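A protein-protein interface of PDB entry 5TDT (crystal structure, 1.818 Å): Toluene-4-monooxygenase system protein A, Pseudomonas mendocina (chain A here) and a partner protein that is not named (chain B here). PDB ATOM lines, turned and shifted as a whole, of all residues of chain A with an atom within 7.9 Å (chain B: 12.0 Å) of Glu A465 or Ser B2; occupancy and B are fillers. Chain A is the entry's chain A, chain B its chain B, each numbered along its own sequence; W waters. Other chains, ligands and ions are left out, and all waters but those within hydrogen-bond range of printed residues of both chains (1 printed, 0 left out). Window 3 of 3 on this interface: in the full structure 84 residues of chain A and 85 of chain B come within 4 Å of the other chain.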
ATOM      1  N   LEU A 393      36.725  10.405  15.559  1.00  0.00           N
ATOM      2  CA  LEU A 393      36.597  11.841  15.294  1.00  0.00           C
ATOM      3  C   LEU A 393      37.802  12.347  14.511  1.00  0.00           C
ATOM      4  O   LEU A 393      38.914  11.838  14.674  1.00  0.00           O
ATOM      5  CB  LEU A 393      36.481  12.649  16.604  1.00  0.00           C
ATOM      6  CG  LEU A 393      35.297  12.304  17.520  1.00  0.00           C
ATOM      7  CD1 LEU A 393      35.138  13.287  18.689  1.00  0.00           C
ATOM      8  CD2 LEU A 393      34.025  12.236  16.706  1.00  0.00           C
ATOM      9  N   PHE A 454      35.577  16.438  24.055  1.00  0.00           N
ATOM     10  CA  PHE A 454      35.404  14.992  23.977  1.00  0.00           C
ATOM     11  C   PHE A 454      36.431  14.275  24.844  1.00  0.00           C
ATOM     12  O   PHE A 454      36.086  13.366  25.611  1.00  0.00           O
ATOM     13  CB  PHE A 454      35.525  14.569  22.514  1.00  0.00           C
ATOM     14  CG  PHE A 454      35.105  13.162  22.237  1.00  0.00           C
ATOM     15  CD1 PHE A 454      33.766  12.826  22.181  1.00  0.00           C
ATOM     16  CD2 PHE A 454      36.049  12.185  21.970  1.00  0.00           C
ATOM     17  CE1 PHE A 454      33.373  11.526  21.906  1.00  0.00           C
ATOM     18  CE2 PHE A 454      35.657  10.881  21.688  1.00  0.00           C
ATOM     19  CZ  PHE A 454      34.320  10.559  21.651  1.00  0.00           C
ATOM     20  N   ILE A 459      31.665  15.369  26.913  1.00  0.00           N
ATOM     21  CA  ILE A 459      30.736  14.797  25.938  1.00  0.00           C
ATOM     22  C   ILE A 459      30.408  13.379  26.396  1.00  0.00           C
ATOM     23  O   ILE A 459      31.223  12.460  26.245  1.00  0.00           O
ATOM     24  CB  ILE A 459      31.302  14.813  24.509  1.00  0.00           C
ATOM     25  CG1 ILE A 459      31.618  16.259  24.064  1.00  0.00           C
ATOM     26  CG2 ILE A 459      30.314  14.150  23.545  1.00  0.00           C
ATOM     27  CD1 ILE A 459      32.192  16.381  22.644  1.00  0.00           C
ATOM     28  N   GLN A 460      29.211  13.196  26.957  1.00  0.00           N
ATOM     29  CA  GLN A 460      28.775  11.897  27.484  1.00  0.00           C
ATOM     30  C   GLN A 460      27.554  11.372  26.733  1.00  0.00           C
ATOM     31  O   GLN A 460      26.591  12.106  26.529  1.00  0.00           O
ATOM     32  CB  GLN A 460      28.469  12.000  28.984  1.00  0.00           C
ATOM     33  CG  GLN A 460      29.679  12.436  29.803  1.00  0.00           C
ATOM     34  CD  GLN A 460      30.803  11.412  29.739  1.00  0.00           C
ATOM     35  OE1 GLN A 460      30.561  10.228  29.467  1.00  0.00           O
ATOM     36  NE2 GLN A 460      32.041  11.861  29.983  1.00  0.00           N
ATOM     37  N   PRO A 461      27.598  10.099  26.309  1.00  0.00           N
ATOM     38  CA  PRO A 461      28.771   9.226  26.435  1.00  0.00           C
ATOM     39  C   PRO A 461      29.891   9.614  25.468  1.00  0.00           C
ATOM     40  O   PRO A 461      29.651  10.307  24.472  1.00  0.00           O
ATOM     41  CB  PRO A 461      28.221   7.832  26.105  1.00  0.00           C
ATOM     42  CG  PRO A 461      26.978   8.062  25.340  1.00  0.00           C
ATOM     43  CD  PRO A 461      26.414   9.375  25.806  1.00  0.00           C
ATOM     44  N   MET A 462      31.114   9.188  25.782  1.00  0.00           N
ATOM     45  CA  MET A 462      32.280   9.502  24.959  1.00  0.00           C
ATOM     46  C   MET A 462      32.329   8.550  23.761  1.00  0.00           C
ATOM     47  O   MET A 462      33.164   7.646  23.663  1.00  0.00           O
ATOM     48  CB  MET A 462      33.548   9.424  25.794  1.00  0.00           C
ATOM     49  CG  MET A 462      34.787   9.987  25.098  1.00  0.00           C
ATOM     50  SD  MET A 462      36.253   9.740  26.109  1.00  0.00           S
ATOM     51  CE  MET A 462      37.512  10.573  25.177  1.00  0.00           C
ATOM     52  N   THR A 463      31.400   8.781  22.835  1.00  0.00           N
ATOM     53  CA  THR A 463      31.225   7.968  21.644  1.00  0.00           C
ATOM     54  C   THR A 463      30.837   8.892  20.501  1.00  0.00           C
ATOM     55  O   THR A 463      30.527  10.068  20.705  1.00  0.00           O
ATOM     56  CB  THR A 463      30.131   6.899  21.822  1.00  0.00           C
ATOM     57  OG1 THR A 463      28.888   7.526  22.166  1.00  0.00           O
ATOM     58  CG2 THR A 463      30.500   5.879  22.909  1.00  0.00           C
ATOM     59  N   LEU A 464      30.807   8.347  19.287  1.00  0.00           N
ATOM     60  CA  LEU A 464      30.350   9.161  18.164  1.00  0.00           C
ATOM     61  C   LEU A 464      28.851   9.439  18.250  1.00  0.00           C
ATOM     62  O   LEU A 464      28.406  10.546  17.933  1.00  0.00           O
ATOM     63  CB  LEU A 464      30.716   8.498  16.838  1.00  0.00           C
ATOM     64  CG  LEU A 464      32.147   8.752  16.347  1.00  0.00           C
ATOM     65  CD1 LEU A 464      33.215   8.256  17.331  1.00  0.00           C
ATOM     66  CD2 LEU A 464      32.344   8.128  14.977  1.00  0.00           C
ATOM     67  N   GLU A 465      28.051   8.471  18.702  1.00  0.00           N
ATOM     68  CA  GLU A 465      26.642   8.786  18.917  1.00  0.00           C
ATOM     69  C   GLU A 465      26.477   9.841  20.009  1.00  0.00           C
ATOM     70  O   GLU A 465      25.663  10.760  19.870  1.00  0.00           O
ATOM     71  CB  GLU A 465      25.837   7.530  19.260  1.00  0.00           C
ATOM     72  CG  GLU A 465      24.325   7.824  19.330  1.00  0.00           C
ATOM     73  CD  GLU A 465      23.466   6.599  19.599  1.00  0.00           C
ATOM     74  OE1 GLU A 465      22.474   6.708  20.361  1.00  0.00           O
ATOM     75  OE2 GLU A 465      23.779   5.525  19.045  1.00  0.00           O
ATOM     76  N   GLY A 466      27.246   9.730  21.100  1.00  0.00           N
ATOM     77  CA  GLY A 466      27.205  10.756  22.135  1.00  0.00           C
ATOM     78  C   GLY A 466      27.588  12.136  21.619  1.00  0.00           C
ATOM     79  O   GLY A 466      26.989  13.145  22.009  1.00  0.00           O
ATOM     80  N   ALA A 467      28.592  12.199  20.740  1.00  0.00           N
ATOM     81  CA  ALA A 467      28.985  13.477  20.151  1.00  0.00           C
ATOM     82  C   ALA A 467      27.868  14.044  19.277  1.00  0.00           C
ATOM     83  O   ALA A 467      27.589  15.247  19.322  1.00  0.00           O
ATOM     84  CB  ALA A 467      30.274  13.310  19.345  1.00  0.00           C
ATOM     85  N   LEU A 468      27.195  13.182  18.506  1.00  0.00           N
ATOM     86  CA  LEU A 468      26.088  13.636  17.669  1.00  0.00           C
ATOM     87  C   LEU A 468      24.954  14.211  18.513  1.00  0.00           C
ATOM     88  O   LEU A 468      24.340  15.214  18.135  1.00  0.00           O
ATOM     89  CB  LEU A 468      25.586  12.484  16.798  1.00  0.00           C
ATOM     90  CG  LEU A 468      26.475  12.176  15.595  1.00  0.00           C
ATOM     91  CD1 LEU A 468      26.186  10.781  15.069  1.00  0.00           C
ATOM     92  CD2 LEU A 468      26.259  13.252  14.510  1.00  0.00           C
ATOM     93  N   LYS A 469      24.663  13.591  19.666  1.00  0.00           N
ATOM     94  CA  LYS A 469      23.640  14.150  20.543  1.00  0.00           C
ATOM     95  C   LYS A 469      24.119  15.448  21.187  1.00  0.00           C
ATOM     96  O   LYS A 469      23.352  16.417  21.289  1.00  0.00           O
ATOM     97  CB  LYS A 469      23.228  13.110  21.590  1.00  0.00           C
ATOM     98  CG  LYS A 469      22.615  11.861  20.945  1.00  0.00           C
ATOM     99  CD  LYS A 469      21.951  10.918  21.956  1.00  0.00           C
ATOM    100  CE  LYS A 469      21.128   9.856  21.224  1.00  0.00           C
ATOM    101  NZ  LYS A 469      20.971   8.607  22.024  1.00  0.00           N
ATOM    102  N   TYR A 470      25.391  15.501  21.594  1.00  0.00           N
ATOM    103  CA  TYR A 470      25.971  16.747  22.091  1.00  0.00           C
ATOM    104  C   TYR A 470      25.853  17.866  21.059  1.00  0.00           C
ATOM    105  O   TYR A 470      25.636  19.033  21.420  1.00  0.00           O
ATOM    106  CB  TYR A 470      27.436  16.520  22.476  1.00  0.00           C
ATOM    107  CG  TYR A 470      28.159  17.762  22.974  1.00  0.00           C
ATOM    108  CD1 TYR A 470      28.000  18.206  24.289  1.00  0.00           C
ATOM    109  CD2 TYR A 470      29.017  18.478  22.139  1.00  0.00           C
ATOM    110  CE1 TYR A 470      28.674  19.327  24.755  1.00  0.00           C
ATOM    111  CE2 TYR A 470      29.693  19.610  22.591  1.00  0.00           C
ATOM    112  CZ  TYR A 470      29.510  20.035  23.890  1.00  0.00           C
ATOM    113  OH  TYR A 470      30.178  21.148  24.351  1.00  0.00           O
ATOM    114  N   MET A 471      26.006  17.533  19.768  1.00  0.00           N
ATOM    115  CA  MET A 471      25.901  18.523  18.693  1.00  0.00           C
ATOM    116  C   MET A 471      24.463  18.969  18.426  1.00  0.00           C
ATOM    117  O   MET A 471      24.254  19.870  17.602  1.00  0.00           O
ATOM    118  CB  MET A 471      26.500  17.972  17.395  1.00  0.00           C
ATOM    119  CG  MET A 471      28.023  17.776  17.397  1.00  0.00           C
ATOM    120  SD  MET A 471      28.613  17.353  15.727  1.00  0.00           S
ATOM    121  CE  MET A 471      30.219  16.638  16.061  1.00  0.00           C
ATOM    122  N   PHE A 473      21.574  17.122  17.469  1.00  0.00           N
ATOM    123  CA  PHE A 473      20.653  16.409  16.603  1.00  0.00           C
ATOM    124  C   PHE A 473      19.565  15.770  17.466  1.00  0.00           C
ATOM    125  O   PHE A 473      19.859  15.005  18.394  1.00  0.00           O
ATOM    126  CB  PHE A 473      21.404  15.376  15.757  1.00  0.00           C
ATOM    127  CG  PHE A 473      22.352  16.008  14.745  1.00  0.00           C
ATOM    128  CD1 PHE A 473      21.858  16.569  13.568  1.00  0.00           C
ATOM    129  CD2 PHE A 473      23.723  16.063  14.983  1.00  0.00           C
ATOM    130  CE1 PHE A 473      22.722  17.175  12.636  1.00  0.00           C
ATOM    131  CE2 PHE A 473      24.596  16.664  14.060  1.00  0.00           C
ATOM    132  CZ  PHE A 473      24.088  17.220  12.879  1.00  0.00           C
ATOM    133  N   ILE A 476      16.891  11.173  14.055  1.00  0.00           N
ATOM    134  CA  ILE A 476      17.704  10.531  13.021  1.00  0.00           C
ATOM    135  C   ILE A 476      17.549  11.216  11.662  1.00  0.00           C
ATOM    136  O   ILE A 476      18.466  11.176  10.831  1.00  0.00           O
ATOM    137  CB  ILE A 476      17.335   9.033  12.945  1.00  0.00           C
ATOM    138  CG1 ILE A 476      18.194   8.297  11.916  1.00  0.00           C
ATOM    139  CG2 ILE A 476      15.841   8.861  12.669  1.00  0.00           C
ATOM    140  CD1 ILE A 476      19.454   7.704  12.511  1.00  0.00           C
ATOM    141  N   MET A 479      20.220  14.289  10.645  1.00  0.00           N
ATOM    142  CA  MET A 479      21.639  14.122  10.339  1.00  0.00           C
ATOM    143  C   MET A 479      21.876  13.935   8.847  1.00  0.00           C
ATOM    144  O   MET A 479      21.061  13.342   8.138  1.00  0.00           O
ATOM    145  CB  MET A 479      22.197  12.943  11.135  1.00  0.00           C
ATOM    146  CG  MET A 479      22.212  13.272  12.611  1.00  0.00           C
ATOM    147  SD  MET A 479      22.789  11.960  13.690  1.00  0.00           S
ATOM    148  CE  MET A 479      21.385  10.874  13.687  1.00  0.00           C
ATOM    149  N   SER B   2      20.710   4.768  19.996  1.00  0.00           N
ATOM    150  CA  SER B   2      19.540   4.933  19.142  1.00  0.00           C
ATOM    151  C   SER B   2      19.055   6.383  19.164  1.00  0.00           C
ATOM    152  O   SER B   2      19.135   7.056  20.196  1.00  0.00           O
ATOM    153  CB  SER B   2      18.419   3.985  19.579  1.00  0.00           C
ATOM    154  N   PHE B   3      18.565   6.856  18.017  1.00  0.00           N
ATOM    155  CA  PHE B   3      17.975   8.181  17.884  1.00  0.00           C
ATOM    156  C   PHE B   3      16.462   8.075  17.735  1.00  0.00           C
ATOM    157  O   PHE B   3      15.959   7.227  16.988  1.00  0.00           O
ATOM    158  CB  PHE B   3      18.545   8.922  16.676  1.00  0.00           C
ATOM    159  CG  PHE B   3      19.884   9.524  16.922  1.00  0.00           C
ATOM    160  CD1 PHE B   3      21.034   8.814  16.635  1.00  0.00           C
ATOM    161  CD2 PHE B   3      19.994  10.803  17.447  1.00  0.00           C
ATOM    162  CE1 PHE B   3      22.275   9.369  16.864  1.00  0.00           C
ATOM    163  CE2 PHE B   3      21.231  11.363  17.679  1.00  0.00           C
ATOM    164  CZ  PHE B   3      22.375  10.644  17.390  1.00  0.00           C
ATOM    165  N   GLU B   4      15.741   8.946  18.436  1.00  0.00           N
ATOM    166  CA  GLU B   4      14.299   9.011  18.274  1.00  0.00           C
ATOM    167  C   GLU B   4      13.946   9.419  16.852  1.00  0.00           C
ATOM    168  O   GLU B   4      14.750  10.004  16.118  1.00  0.00           O
ATOM    169  CB  GLU B   4      13.683  10.003  19.259  1.00  0.00           C
ATOM    170  CG  GLU B   4      13.880   9.634  20.714  1.00  0.00           C
ATOM    171  CD  GLU B   4      13.198  10.608  21.651  1.00  0.00           C
ATOM    172  OE1 GLU B   4      13.094  11.800  21.290  1.00  0.00           O
ATOM    173  OE2 GLU B   4      12.766  10.184  22.745  1.00  0.00           O
ATOM    174  N   SER B   5      12.719   9.112  16.461  1.00  0.00           N
ATOM    175  CA  SER B   5      12.210   9.557  15.177  1.00  0.00           C
ATOM    176  C   SER B   5      11.249  10.708  15.410  1.00  0.00           C
ATOM    177  O   SER B   5      10.516  10.725  16.404  1.00  0.00           O
ATOM    178  CB  SER B   5      11.517   8.424  14.428  1.00  0.00           C
ATOM    179  OG  SER B   5      11.439   8.727  13.048  1.00  0.00           O
ATOM    180  N   LYS B   6      11.289  11.691  14.515  1.00  0.00           N
ATOM    181  CA  LYS B   6      10.385  12.821  14.613  1.00  0.00           C
ATOM    182  C   LYS B   6      10.050  13.286  13.207  1.00  0.00           C
ATOM    183  O   LYS B   6      10.859  13.156  12.284  1.00  0.00           O
ATOM    184  CB  LYS B   6      10.987  13.966  15.435  1.00  0.00           C
ATOM    185  CG  LYS B   6      10.986  13.726  16.939  1.00  0.00           C
ATOM    186  CD  LYS B   6      11.590  14.911  17.662  1.00  0.00           C
ATOM    187  CE  LYS B   6      11.919  14.578  19.105  1.00  0.00           C
ATOM    188  NZ  LYS B   6      12.580  15.721  19.789  1.00  0.00           N
HETATM  189  O   HOH W   1      17.917   9.383  22.025  1.00  0.00           O
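Water W1 lies within hydrogen-bond range of the side-chain amino group of Lys A469 (3.2 Å) and the backbone carbonyl oxygen of Ser B2 (3.2 Å).
Among the printed residues, merely in contact across the chains: Glu A465 with Phe B3 (3.6 Å), Lys A469 with Phe B3 (3.6 Å), Met A479 with Phe B3 (3.6 Å), Leu A468 with Phe B3 (3.7 Å), Ile A476 with Phe B3 (3.8 Å) and Phe A473 with Phe B3 (3.96 Å).
Hydrophobic or aromatic side chains of chain A within 4 Å of the printed part of chain B: Leu A468, Ile A476 and Met A479. Along chain B the printed residues that touch a printed residue of chain A span positions 2 to 4. Among the printed residues, no Asp or Glu carboxylate lies within 4 Å of a Lys or Arg side-chain nitrogen of the other chain.
Of chain B, only Ser B2 and Phe B3 come within 4 Å of Glu A465. Ser B2 touches just these residues of chain A: Glu A465 (2.6 Å) and Lys A469 (3.0 Å). No residue of chain B comes within 4 Å of Pro A461. Leu A464 touches none of the printed residues of chain B. Gly A466 touches none of the printed residues of chain B. No residue of chain B comes within 4 Å of Ala A467. Printed residues of chain B within 4 Å of Leu A468: Phe B3. Lys A469 touches just these residues of chain B: Ser B2 (3.0 Å) and Phe B3 (3.6 Å). Printed residues of chain B within 4 Å of Met A479: Phe B3. Of the printed residues of chain A, Phe B3 touches Glu A465 (3.6 Å), Leu A468 (3.7 Å), Lys A469 (3.6 Å), Phe A473 (3.96 Å), Ile A476 (3.8 Å) and Met A479 (3.6 Å). Ser B5 touches none of the printed residues of chain A. Met A462 touches none of the printed residues of chain B. The nearest residue of chain B that does not touch Glu A465 is Glu B4 (7.4 Å). The nearest printed residue of chain B that does not touch Ile A476 is Ser B5 (4.4 Å).
O of Ser B2 is in hydrogen-bond range of NZ of Lys A469 (3.0 Å). The backbone NH (N) of Ser B2 sits at hydrogen-bond distance from the side-chain carboxylate (OE1) of Glu A465, 2.6 Å away. N of Ile A476 sits at hydrogen-bond distance from O of Glu B4, 3.2 Å away.
The backbone NH (N) of Phe A473 lies close to the backbone carbonyl oxygen (O) of Leu A468 (3.4 Å). The side-chain carboxylate of Glu A465 is in salt-bridge range of the side-chain amino group of Lys A469 (2.9 Å).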
